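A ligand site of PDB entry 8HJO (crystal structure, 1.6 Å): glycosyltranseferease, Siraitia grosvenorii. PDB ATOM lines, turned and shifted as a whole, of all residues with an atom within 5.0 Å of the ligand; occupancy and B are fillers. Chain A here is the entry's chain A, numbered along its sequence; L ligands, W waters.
An oxygen (O7) of the ligand sits at hydrogen-bond distance from the side-chain hydroxyl (OG) of Ser 355, 2.6 Å away.
OG of Ser 272 is in hydrogen-bond range of O12 of the ligand (2.6 Å).
NE2 of His 350 is in hydrogen-bond range of O10 of the ligand (2.8 Å).
The backbone NH (N) of Ala 333 is in hydrogen-bond range of an oxygen (O2) of the ligand.
ND2 of Asn 354 is in hydrogen-bond range of O8 of the ligand (2.9 Å).
The backbone carbonyl oxygen of Ala 333 lies within hydrogen-bond range of a nitrogen (N2) of the ligand (2.8 Å).
N of Asn 354 sits at hydrogen-bond distance from O8 of the ligand, at 3.0 Å.
An oxygen (O8) of the ligand sits at hydrogen-bond distance from the backbone NH of Trp 353, at 3.4 Å.
The backbone NH (N) of Ser 355 is in hydrogen-bond range of an oxygen (O7) of the ligand (2.9 Å).
OE2 of Glu 358 is in hydrogen-bond range of O5 of the ligand (2.6 Å).
An oxygen (O12) of the ligand sits at hydrogen-bond distance from the backbone NH (N) of Ser 272, 2.7 Å away.
NE2 of Gln 335 sits at hydrogen-bond distance from O3 of the ligand (3.1 Å).
The backbone NH (N) of His 350 sits at hydrogen-bond distance from the backbone carbonyl oxygen (O) of Ser 269, at 3.3 Å.
OG of Ser 269 sits at hydrogen-bond distance from N of Gly 271, at 3.2 Å.
The backbone carbonyl oxygen (O) of Gly 21 lies within hydrogen-bond range of the side-chain amide nitrogen (ND2) of Asn 354 (3.1 Å).
The side-chain carboxylate (OE1) of Glu 358 lies within hydrogen-bond range of the side-chain amide nitrogen (NE2) of Gln 335 (2.8 Å).
OG of Ser 24 is in hydrogen-bond range of O of Tyr 20 (2.7 Å).
NE2 of Gln 335 is in hydrogen-bond range of OG of Ser 355 (3.1 Å).
A ring nitrogen (ND1) of His 350 lies close to the backbone NH of Gly 352 (3.4 Å).
CD2 of Tyr 20 touches O4 of the ligand, at 3.4 Å.
Gly 21 touches the ligand (CA to O6, 3.9 Å).
Ser 269 touches the ligand (OG to C3, 3.7 Å).
Gly 271 touches the ligand (C to O12, 3.7 Å).
CG of Glu 273 touches O10 of the ligand (3.8 Å).
CG1 of Val 298 touches O2 of the ligand, at 3.7 Å.
Trp 332 touches the ligand.
Gly 352 touches the ligand (C to O7, 3.5 Å).
Hydrophobic or aromatic side chains that line the ligand: Tyr 20, Val 298, Trp 332 and His 350.
16 residues have an atom within 4 Å of the ligand: Tyr 20, Gly 21, Ser 269, Gly 271, Ser 272, Glu 273, Val 298, Trp 332, Ala 333, Gln 335, His 350, Gly 352, Trp 353, Asn 354, Ser 355 and Glu 358.
The nearest printed residue that does not touch the ligand is Gln 375 (4.4 Å).
Water W7 lies within hydrogen-bond range of an oxygen (O10) of the ligand (2.5 Å) and the side-chain amide nitrogen (NE2) of Gln 375 (3.5 Å).
Water W3 lies within hydrogen-bond range of an oxygen (O10) of the ligand (2.6 Å), the backbone NH (N) of Glu 273 (2.9 Å), the backbone carbonyl oxygen (O) of Phe 270 (2.9 Å), the backbone NH (N) of Ser 272 (3.4 Å) and a ring nitrogen (NE2) of His 350 (3.5 Å).
Water W1 bridges an oxygen (O1) of the ligand and the indole nitrogen of Trp 332.
Water W6 lies within hydrogen-bond range of OE1 of Glu 273, O11 of the ligand, N of Gly 21 and N of Tyr 20.
Water W5 lies within hydrogen-bond range of the side-chain hydroxyl (OG) of Ser 269, the side-chain amide oxygen (OE1) of Gln 335, the side-chain hydroxyl (OG) of Ser 355 and the backbone NH (N) of Gly 271.
Water W4 lies within hydrogen-bond range of N of Ala 336 (2.8 Å), N of Gln 335 (3.5 Å) and O1 of the ligand (3.5 Å).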
ATOM      1  N   TYR A  20      -4.985   2.178 -23.452  1.00  0.00           N
ATOM      2  CA  TYR A  20      -6.143   1.890 -24.301  1.00  0.00           C
ATOM      3  C   TYR A  20      -6.942   0.678 -23.813  1.00  0.00           C
ATOM      4  O   TYR A  20      -8.173   0.688 -23.840  1.00  0.00           O
ATOM      5  CB  TYR A  20      -5.706   1.678 -25.744  1.00  0.00           C
ATOM      6  CG  TYR A  20      -6.871   1.508 -26.701  1.00  0.00           C
ATOM      7  CD1 TYR A  20      -7.510   2.604 -27.257  1.00  0.00           C
ATOM      8  CD2 TYR A  20      -7.328   0.235 -27.040  1.00  0.00           C
ATOM      9  CE1 TYR A  20      -8.580   2.448 -28.138  1.00  0.00           C
ATOM     10  CE2 TYR A  20      -8.395   0.063 -27.896  1.00  0.00           C
ATOM     11  CZ  TYR A  20      -9.017   1.172 -28.445  1.00  0.00           C
ATOM     12  OH  TYR A  20     -10.070   0.990 -29.329  1.00  0.00           O
ATOM     13  N   GLY A  21      -6.246  -0.386 -23.394  1.00  0.00           N
ATOM     14  CA  GLY A  21      -6.945  -1.558 -22.889  1.00  0.00           C
ATOM     15  C   GLY A  21      -7.729  -1.259 -21.628  1.00  0.00           C
ATOM     16  O   GLY A  21      -8.825  -1.788 -21.427  1.00  0.00           O
ATOM     17  N   SER A  24     -10.740   0.824 -22.623  1.00  0.00           N
ATOM     18  CA  SER A  24     -11.726  -0.003 -23.297  1.00  0.00           C
ATOM     19  C   SER A  24     -12.569  -0.777 -22.301  1.00  0.00           C
ATOM     20  O   SER A  24     -13.805  -0.800 -22.391  1.00  0.00           O
ATOM     21  CB  SER A  24     -11.037  -0.967 -24.263  1.00  0.00           C
ATOM     22  OG  SER A  24     -10.291  -0.262 -25.247  1.00  0.00           O
ATOM     23  N   PHE A 267      -4.332 -13.889 -36.874  1.00  0.00           N
ATOM     24  CA  PHE A 267      -4.080 -12.480 -36.601  1.00  0.00           C
ATOM     25  C   PHE A 267      -2.912 -12.417 -35.622  1.00  0.00           C
ATOM     26  O   PHE A 267      -2.778 -13.275 -34.746  1.00  0.00           O
ATOM     27  CB  PHE A 267      -5.344 -11.862 -35.994  1.00  0.00           C
ATOM     28  CG  PHE A 267      -5.234 -10.397 -35.691  1.00  0.00           C
ATOM     29  CD1 PHE A 267      -5.011  -9.475 -36.702  1.00  0.00           C
ATOM     30  CD2 PHE A 267      -5.368  -9.937 -34.394  1.00  0.00           C
ATOM     31  CE1 PHE A 267      -4.919  -8.124 -36.437  1.00  0.00           C
ATOM     32  CE2 PHE A 267      -5.298  -8.583 -34.109  1.00  0.00           C
ATOM     33  CZ  PHE A 267      -5.077  -7.678 -35.125  1.00  0.00           C
ATOM     34  N   SER A 269      -0.838  -9.765 -33.144  1.00  0.00           N
ATOM     35  CA  SER A 269      -0.868  -8.420 -32.571  1.00  0.00           C
ATOM     36  C   SER A 269      -0.227  -8.464 -31.211  1.00  0.00           C
ATOM     37  O   SER A 269      -0.437  -9.419 -30.452  1.00  0.00           O
ATOM     38  CB  SER A 269      -2.301  -7.880 -32.447  1.00  0.00           C
ATOM     39  OG  SER A 269      -2.328  -6.670 -31.678  1.00  0.00           O
ATOM     40  N   PHE A 270       0.535  -7.424 -30.875  1.00  0.00           N
ATOM     41  CA  PHE A 270       1.086  -7.323 -29.534  1.00  0.00           C
ATOM     42  C   PHE A 270       0.467  -6.175 -28.739  1.00  0.00           C
ATOM     43  O   PHE A 270       1.081  -5.655 -27.806  1.00  0.00           O
ATOM     44  CB  PHE A 270       2.597  -7.218 -29.612  1.00  0.00           C
ATOM     45  CG  PHE A 270       3.208  -8.433 -30.209  1.00  0.00           C
ATOM     46  CD1 PHE A 270       3.368  -9.581 -29.435  1.00  0.00           C
ATOM     47  CD2 PHE A 270       3.511  -8.488 -31.559  1.00  0.00           C
ATOM     48  CE1 PHE A 270       3.873 -10.739 -30.005  1.00  0.00           C
ATOM     49  CE2 PHE A 270       4.031  -9.645 -32.119  1.00  0.00           C
ATOM     50  CZ  PHE A 270       4.204 -10.759 -31.345  1.00  0.00           C
ATOM     51  N   GLY A 271      -0.762  -5.799 -29.063  1.00  0.00           N
ATOM     52  CA  GLY A 271      -1.485  -4.880 -28.218  1.00  0.00           C
ATOM     53  C   GLY A 271      -1.151  -3.436 -28.552  1.00  0.00           C
ATOM     54  O   GLY A 271      -0.583  -3.111 -29.605  1.00  0.00           O
ATOM     55  N   SER A 272      -1.489  -2.563 -27.611  1.00  0.00           N
ATOM     56  CA  SER A 272      -1.390  -1.136 -27.839  1.00  0.00           C
ATOM     57  C   SER A 272      -0.171  -0.502 -27.198  1.00  0.00           C
ATOM     58  O   SER A 272       0.081   0.682 -27.422  1.00  0.00           O
ATOM     59  CB  SER A 272      -2.645  -0.431 -27.310  1.00  0.00           C
ATOM     60  OG  SER A 272      -2.700  -0.515 -25.885  1.00  0.00           O
ATOM     61  N   GLU A 273       0.602  -1.240 -26.398  1.00  0.00           N
ATOM     62  CA  GLU A 273       1.680  -0.583 -25.666  1.00  0.00           C
ATOM     63  C   GLU A 273       2.923  -1.463 -25.589  1.00  0.00           C
ATOM     64  O   GLU A 273       3.633  -1.477 -24.584  1.00  0.00           O
ATOM     65  CB  GLU A 273       1.214  -0.128 -24.274  1.00  0.00           C
ATOM     66  CG  GLU A 273       0.392  -1.097 -23.491  1.00  0.00           C
ATOM     67  CD  GLU A 273       0.108  -0.575 -22.072  1.00  0.00           C
ATOM     68  OE1 GLU A 273      -0.961   0.047 -21.838  1.00  0.00           O
ATOM     69  OE2 GLU A 273       0.968  -0.780 -21.193  1.00  0.00           O
ATOM     70  N   VAL A 298      -0.120  -6.876 -37.299  1.00  0.00           N
ATOM     71  CA  VAL A 298      -0.080  -5.443 -37.016  1.00  0.00           C
ATOM     72  C   VAL A 298       1.312  -5.085 -36.549  1.00  0.00           C
ATOM     73  O   VAL A 298       1.782  -5.592 -35.527  1.00  0.00           O
ATOM     74  CB  VAL A 298      -1.124  -5.050 -35.963  1.00  0.00           C
ATOM     75  CG1 VAL A 298      -1.027  -3.537 -35.684  1.00  0.00           C
ATOM     76  CG2 VAL A 298      -2.500  -5.438 -36.400  1.00  0.00           C
ATOM     77  N   GLY A 331       0.328   0.216 -37.851  1.00  0.00           N
ATOM     78  CA  GLY A 331      -0.321   1.072 -36.875  1.00  0.00           C
ATOM     79  C   GLY A 331      -1.451   0.454 -36.072  1.00  0.00           C
ATOM     80  O   GLY A 331      -1.374   0.364 -34.837  1.00  0.00           O
ATOM     81  N   TRP A 332      -2.518   0.040 -36.741  1.00  0.00           N
ATOM     82  CA  TRP A 332      -3.719  -0.373 -36.018  1.00  0.00           C
ATOM     83  C   TRP A 332      -4.612  -1.144 -36.972  1.00  0.00           C
ATOM     84  O   TRP A 332      -4.698  -0.805 -38.156  1.00  0.00           O
ATOM     85  CB  TRP A 332      -4.468   0.832 -35.455  1.00  0.00           C
ATOM     86  CG  TRP A 332      -5.457   0.529 -34.343  1.00  0.00           C
ATOM     87  CD1 TRP A 332      -6.814   0.422 -34.458  1.00  0.00           C
ATOM     88  CD2 TRP A 332      -5.159   0.368 -32.948  1.00  0.00           C
ATOM     89  NE1 TRP A 332      -7.380   0.175 -33.219  1.00  0.00           N
ATOM     90  CE2 TRP A 332      -6.384   0.151 -32.283  1.00  0.00           C
ATOM     91  CE3 TRP A 332      -3.976   0.366 -32.201  1.00  0.00           C
ATOM     92  CZ2 TRP A 332      -6.448  -0.082 -30.907  1.00  0.00           C
ATOM     93  CZ3 TRP A 332      -4.050   0.163 -30.834  1.00  0.00           C
ATOM     94  CH2 TRP A 332      -5.289  -0.060 -30.198  1.00  0.00           C
ATOM     95  N   ALA A 333      -5.281  -2.179 -36.468  1.00  0.00           N
ATOM     96  CA  ALA A 333      -6.206  -2.955 -37.263  1.00  0.00           C
ATOM     97  C   ALA A 333      -7.502  -3.158 -36.495  1.00  0.00           C
ATOM     98  O   ALA A 333      -7.537  -3.016 -35.273  1.00  0.00           O
ATOM     99  CB  ALA A 333      -5.608  -4.313 -37.651  1.00  0.00           C
ATOM    100  N   PRO A 334      -8.593  -3.459 -37.196  1.00  0.00           N
ATOM    101  CA  PRO A 334      -9.881  -3.797 -36.524  1.00  0.00           C
ATOM    102  C   PRO A 334      -9.848  -5.212 -35.960  1.00  0.00           C
ATOM    103  O   PRO A 334     -10.316  -6.191 -36.542  1.00  0.00           O
ATOM    104  CB  PRO A 334     -10.900  -3.630 -37.669  1.00  0.00           C
ATOM    105  CG  PRO A 334     -10.113  -3.904 -38.896  1.00  0.00           C
ATOM    106  CD  PRO A 334      -8.737  -3.367 -38.659  1.00  0.00           C
ATOM    107  N   GLN A 335      -9.275  -5.336 -34.751  1.00  0.00           N
ATOM    108  CA  GLN A 335      -8.989  -6.653 -34.192  1.00  0.00           C
ATOM    109  C   GLN A 335     -10.257  -7.489 -34.040  1.00  0.00           C
ATOM    110  O   GLN A 335     -10.276  -8.675 -34.408  1.00  0.00           O
ATOM    111  CB  GLN A 335      -8.301  -6.499 -32.839  1.00  0.00           C
ATOM    112  CG  GLN A 335      -8.140  -7.816 -32.078  1.00  0.00           C
ATOM    113  CD  GLN A 335      -7.093  -7.729 -30.967  1.00  0.00           C
ATOM    114  OE1 GLN A 335      -6.025  -7.156 -31.160  1.00  0.00           O
ATOM    115  NE2 GLN A 335      -7.388  -8.292 -29.800  1.00  0.00           N
ATOM    116  N   ALA A 336     -11.319  -6.912 -33.480  1.00  0.00           N
ATOM    117  CA  ALA A 336     -12.519  -7.715 -33.205  1.00  0.00           C
ATOM    118  C   ALA A 336     -13.176  -8.186 -34.495  1.00  0.00           C
ATOM    119  O   ALA A 336     -13.649  -9.311 -34.575  1.00  0.00           O
ATOM    120  CB  ALA A 336     -13.514  -6.923 -32.365  1.00  0.00           C
ATOM    121  N   HIS A 350       0.072 -11.264 -27.718  1.00  0.00           N
ATOM    122  CA  HIS A 350       0.874 -11.002 -26.516  1.00  0.00           C
ATOM    123  C   HIS A 350       0.132 -11.398 -25.249  1.00  0.00           C
ATOM    124  O   HIS A 350       0.739 -11.378 -24.168  1.00  0.00           O
ATOM    125  CB  HIS A 350       1.306  -9.522 -26.426  1.00  0.00           C
ATOM    126  CG  HIS A 350       0.212  -8.562 -26.051  1.00  0.00           C
ATOM    127  ND1 HIS A 350      -1.060  -8.594 -26.587  1.00  0.00           N
ATOM    128  CD2 HIS A 350       0.222  -7.501 -25.187  1.00  0.00           C
ATOM    129  CE1 HIS A 350      -1.798  -7.632 -26.056  1.00  0.00           C
ATOM    130  NE2 HIS A 350      -1.041  -6.952 -25.206  1.00  0.00           N
ATOM    131  N   GLY A 352      -2.359  -9.869 -23.717  1.00  0.00           N
ATOM    132  CA  GLY A 352      -3.093  -8.861 -22.981  1.00  0.00           C
ATOM    133  C   GLY A 352      -4.492  -9.345 -22.679  1.00  0.00           C
ATOM    134  O   GLY A 352      -5.099 -10.105 -23.437  1.00  0.00           O
ATOM    135  N   TRP A 353      -5.028  -8.908 -21.540  1.00  0.00           N
ATOM    136  CA  TRP A 353      -6.250  -9.558 -21.070  1.00  0.00           C
ATOM    137  C   TRP A 353      -7.459  -9.255 -21.947  1.00  0.00           C
ATOM    138  O   TRP A 353      -8.347 -10.122 -22.101  1.00  0.00           O
ATOM    139  CB  TRP A 353      -6.533  -9.156 -19.626  1.00  0.00           C
ATOM    140  CG  TRP A 353      -7.577 -10.013 -18.995  1.00  0.00           C
ATOM    141  CD1 TRP A 353      -8.794  -9.610 -18.555  1.00  0.00           C
ATOM    142  CD2 TRP A 353      -7.516 -11.434 -18.805  1.00  0.00           C
ATOM    143  NE1 TRP A 353      -9.493 -10.694 -18.056  1.00  0.00           N
ATOM    144  CE2 TRP A 353      -8.725 -11.822 -18.204  1.00  0.00           C
ATOM    145  CE3 TRP A 353      -6.542 -12.411 -19.056  1.00  0.00           C
ATOM    146  CZ2 TRP A 353      -9.003 -13.144 -17.856  1.00  0.00           C
ATOM    147  CZ3 TRP A 353      -6.825 -13.728 -18.720  1.00  0.00           C
ATOM    148  CH2 TRP A 353      -8.036 -14.082 -18.129  1.00  0.00           C
ATOM    149  N   ASN A 354      -7.543  -8.061 -22.528  1.00  0.00           N
ATOM    150  CA  ASN A 354      -8.673  -7.801 -23.405  1.00  0.00           C
ATOM    151  C   ASN A 354      -8.605  -8.687 -24.637  1.00  0.00           C
ATOM    152  O   ASN A 354      -9.629  -9.203 -25.099  1.00  0.00           O
ATOM    153  CB  ASN A 354      -8.729  -6.334 -23.807  1.00  0.00           C
ATOM    154  CG  ASN A 354      -9.017  -5.436 -22.635  1.00  0.00           C
ATOM    155  OD1 ASN A 354     -10.112  -5.448 -22.086  1.00  0.00           O
ATOM    156  ND2 ASN A 354      -8.009  -4.677 -22.223  1.00  0.00           N
ATOM    157  N   SER A 355      -7.397  -8.859 -25.186  1.00  0.00           N
ATOM    158  CA  SER A 355      -7.224  -9.759 -26.333  1.00  0.00           C
ATOM    159  C   SER A 355      -7.599 -11.190 -25.981  1.00  0.00           C
ATOM    160  O   SER A 355      -8.216 -11.882 -26.790  1.00  0.00           O
ATOM    161  CB  SER A 355      -5.783  -9.687 -26.858  1.00  0.00           C
ATOM    162  OG  SER A 355      -5.491  -8.384 -27.358  1.00  0.00           O
ATOM    163  N   GLU A 358     -11.461 -11.317 -25.710  1.00  0.00           N
ATOM    164  CA  GLU A 358     -12.033 -11.242 -27.050  1.00  0.00           C
ATOM    165  C   GLU A 358     -11.868 -12.565 -27.769  1.00  0.00           C
ATOM    166  O   GLU A 358     -12.822 -13.069 -28.373  1.00  0.00           O
ATOM    167  CB  GLU A 358     -11.351 -10.123 -27.841  1.00  0.00           C
ATOM    168  CG  GLU A 358     -11.781  -8.738 -27.393  1.00  0.00           C
ATOM    169  CD  GLU A 358     -10.842  -7.635 -27.864  1.00  0.00           C
ATOM    170  OE1 GLU A 358      -9.948  -7.913 -28.696  1.00  0.00           O
ATOM    171  OE2 GLU A 358     -11.004  -6.489 -27.385  1.00  0.00           O
ATOM    172  N   GLN A 375       1.211 -10.443 -18.866  1.00  0.00           N
ATOM    173  CA  GLN A 375       1.022 -11.362 -19.986  1.00  0.00           C
ATOM    174  C   GLN A 375       1.503 -12.788 -19.745  1.00  0.00           C
ATOM    175  O   GLN A 375       0.781 -13.724 -20.134  1.00  0.00           O
ATOM    176  CB  GLN A 375       1.682 -10.768 -21.237  1.00  0.00           C
ATOM    177  CG  GLN A 375       1.013  -9.459 -21.719  1.00  0.00           C
ATOM    178  CD  GLN A 375       1.979  -8.467 -22.346  1.00  0.00           C
ATOM    179  OE1 GLN A 375       3.008  -8.858 -22.929  1.00  0.00           O
ATOM    180  NE2 GLN A 375       1.676  -7.175 -22.208  1.00  0.00           N
HETATM  181  N1  LIG L   1      -6.521  -3.483 -30.512  1.00  0.00           N
HETATM  182  C1  LIG L   1      -7.085  -3.215 -31.732  1.00  0.00           C
HETATM  183  N2  LIG L   1      -6.214  -3.148 -32.823  1.00  0.00           N
HETATM  184  C2  LIG L   1      -4.853  -3.320 -32.761  1.00  0.00           C
HETATM  185  C3  LIG L   1      -4.328  -3.592 -31.455  1.00  0.00           C
HETATM  186  C4  LIG L   1      -5.157  -3.669 -30.373  1.00  0.00           C
HETATM  187  O1  LIG L   1      -8.288  -3.052 -31.879  1.00  0.00           O
HETATM  188  O2  LIG L   1      -4.203  -3.236 -33.798  1.00  0.00           O
HETATM  189  C5  LIG L   1      -7.400  -3.546 -29.339  1.00  0.00           C
HETATM  190  C6  LIG L   1      -7.675  -5.010 -28.865  1.00  0.00           C
HETATM  191  O3  LIG L   1      -8.832  -5.528 -29.532  1.00  0.00           O
HETATM  192  C7  LIG L   1      -7.917  -4.836 -27.386  1.00  0.00           C
HETATM  193  C8  LIG L   1      -7.004  -3.664 -27.021  1.00  0.00           C
HETATM  194  O4  LIG L   1      -6.722  -2.926 -28.261  1.00  0.00           O
HETATM  195  O5  LIG L   1      -9.292  -4.491 -27.102  1.00  0.00           O
HETATM  196  C9  LIG L   1      -5.723  -4.177 -26.501  1.00  0.00           C
HETATM  197  O6  LIG L   1      -5.955  -4.553 -25.151  1.00  0.00           O
HETATM  198  P1  LIG L   1      -5.054  -5.739 -24.472  1.00  0.00           P
HETATM  199  O7  LIG L   1      -5.110  -7.020 -25.228  1.00  0.00           O
HETATM  200  O8  LIG L   1      -5.541  -5.879 -23.059  1.00  0.00           O
HETATM  201  O9  LIG L   1      -3.480  -5.335 -24.515  1.00  0.00           O
HETATM  202  P2  LIG L   1      -2.708  -3.932 -24.141  1.00  0.00           P
HETATM  203  O10 LIG L   1      -1.309  -4.458 -23.892  1.00  0.00           O
HETATM  204  O11 LIG L   1      -3.316  -3.351 -22.886  1.00  0.00           O
HETATM  205  O12 LIG L   1      -2.848  -3.014 -25.296  1.00  0.00           O
HETATM  206  O   HOH W   1     -10.044  -1.478 -33.200  1.00  0.00           O
HETATM  207  O   HOH W   2     -11.272  -2.900 -27.429  1.00  0.00           O
HETATM  208  O   HOH W   3       0.709  -3.973 -25.497  1.00  0.00           O
HETATM  209  O   HOH W   4     -11.436  -4.424 -32.221  1.00  0.00           O
HETATM  210  O   HOH W   5      -3.930  -6.803 -29.638  1.00  0.00           O
HETATM  211  O   HOH W   6      -3.499  -0.652 -22.356  1.00  0.00           O
HETATM  212  O   HOH W   7      -0.135  -4.261 -21.650  1.00  0.00           O
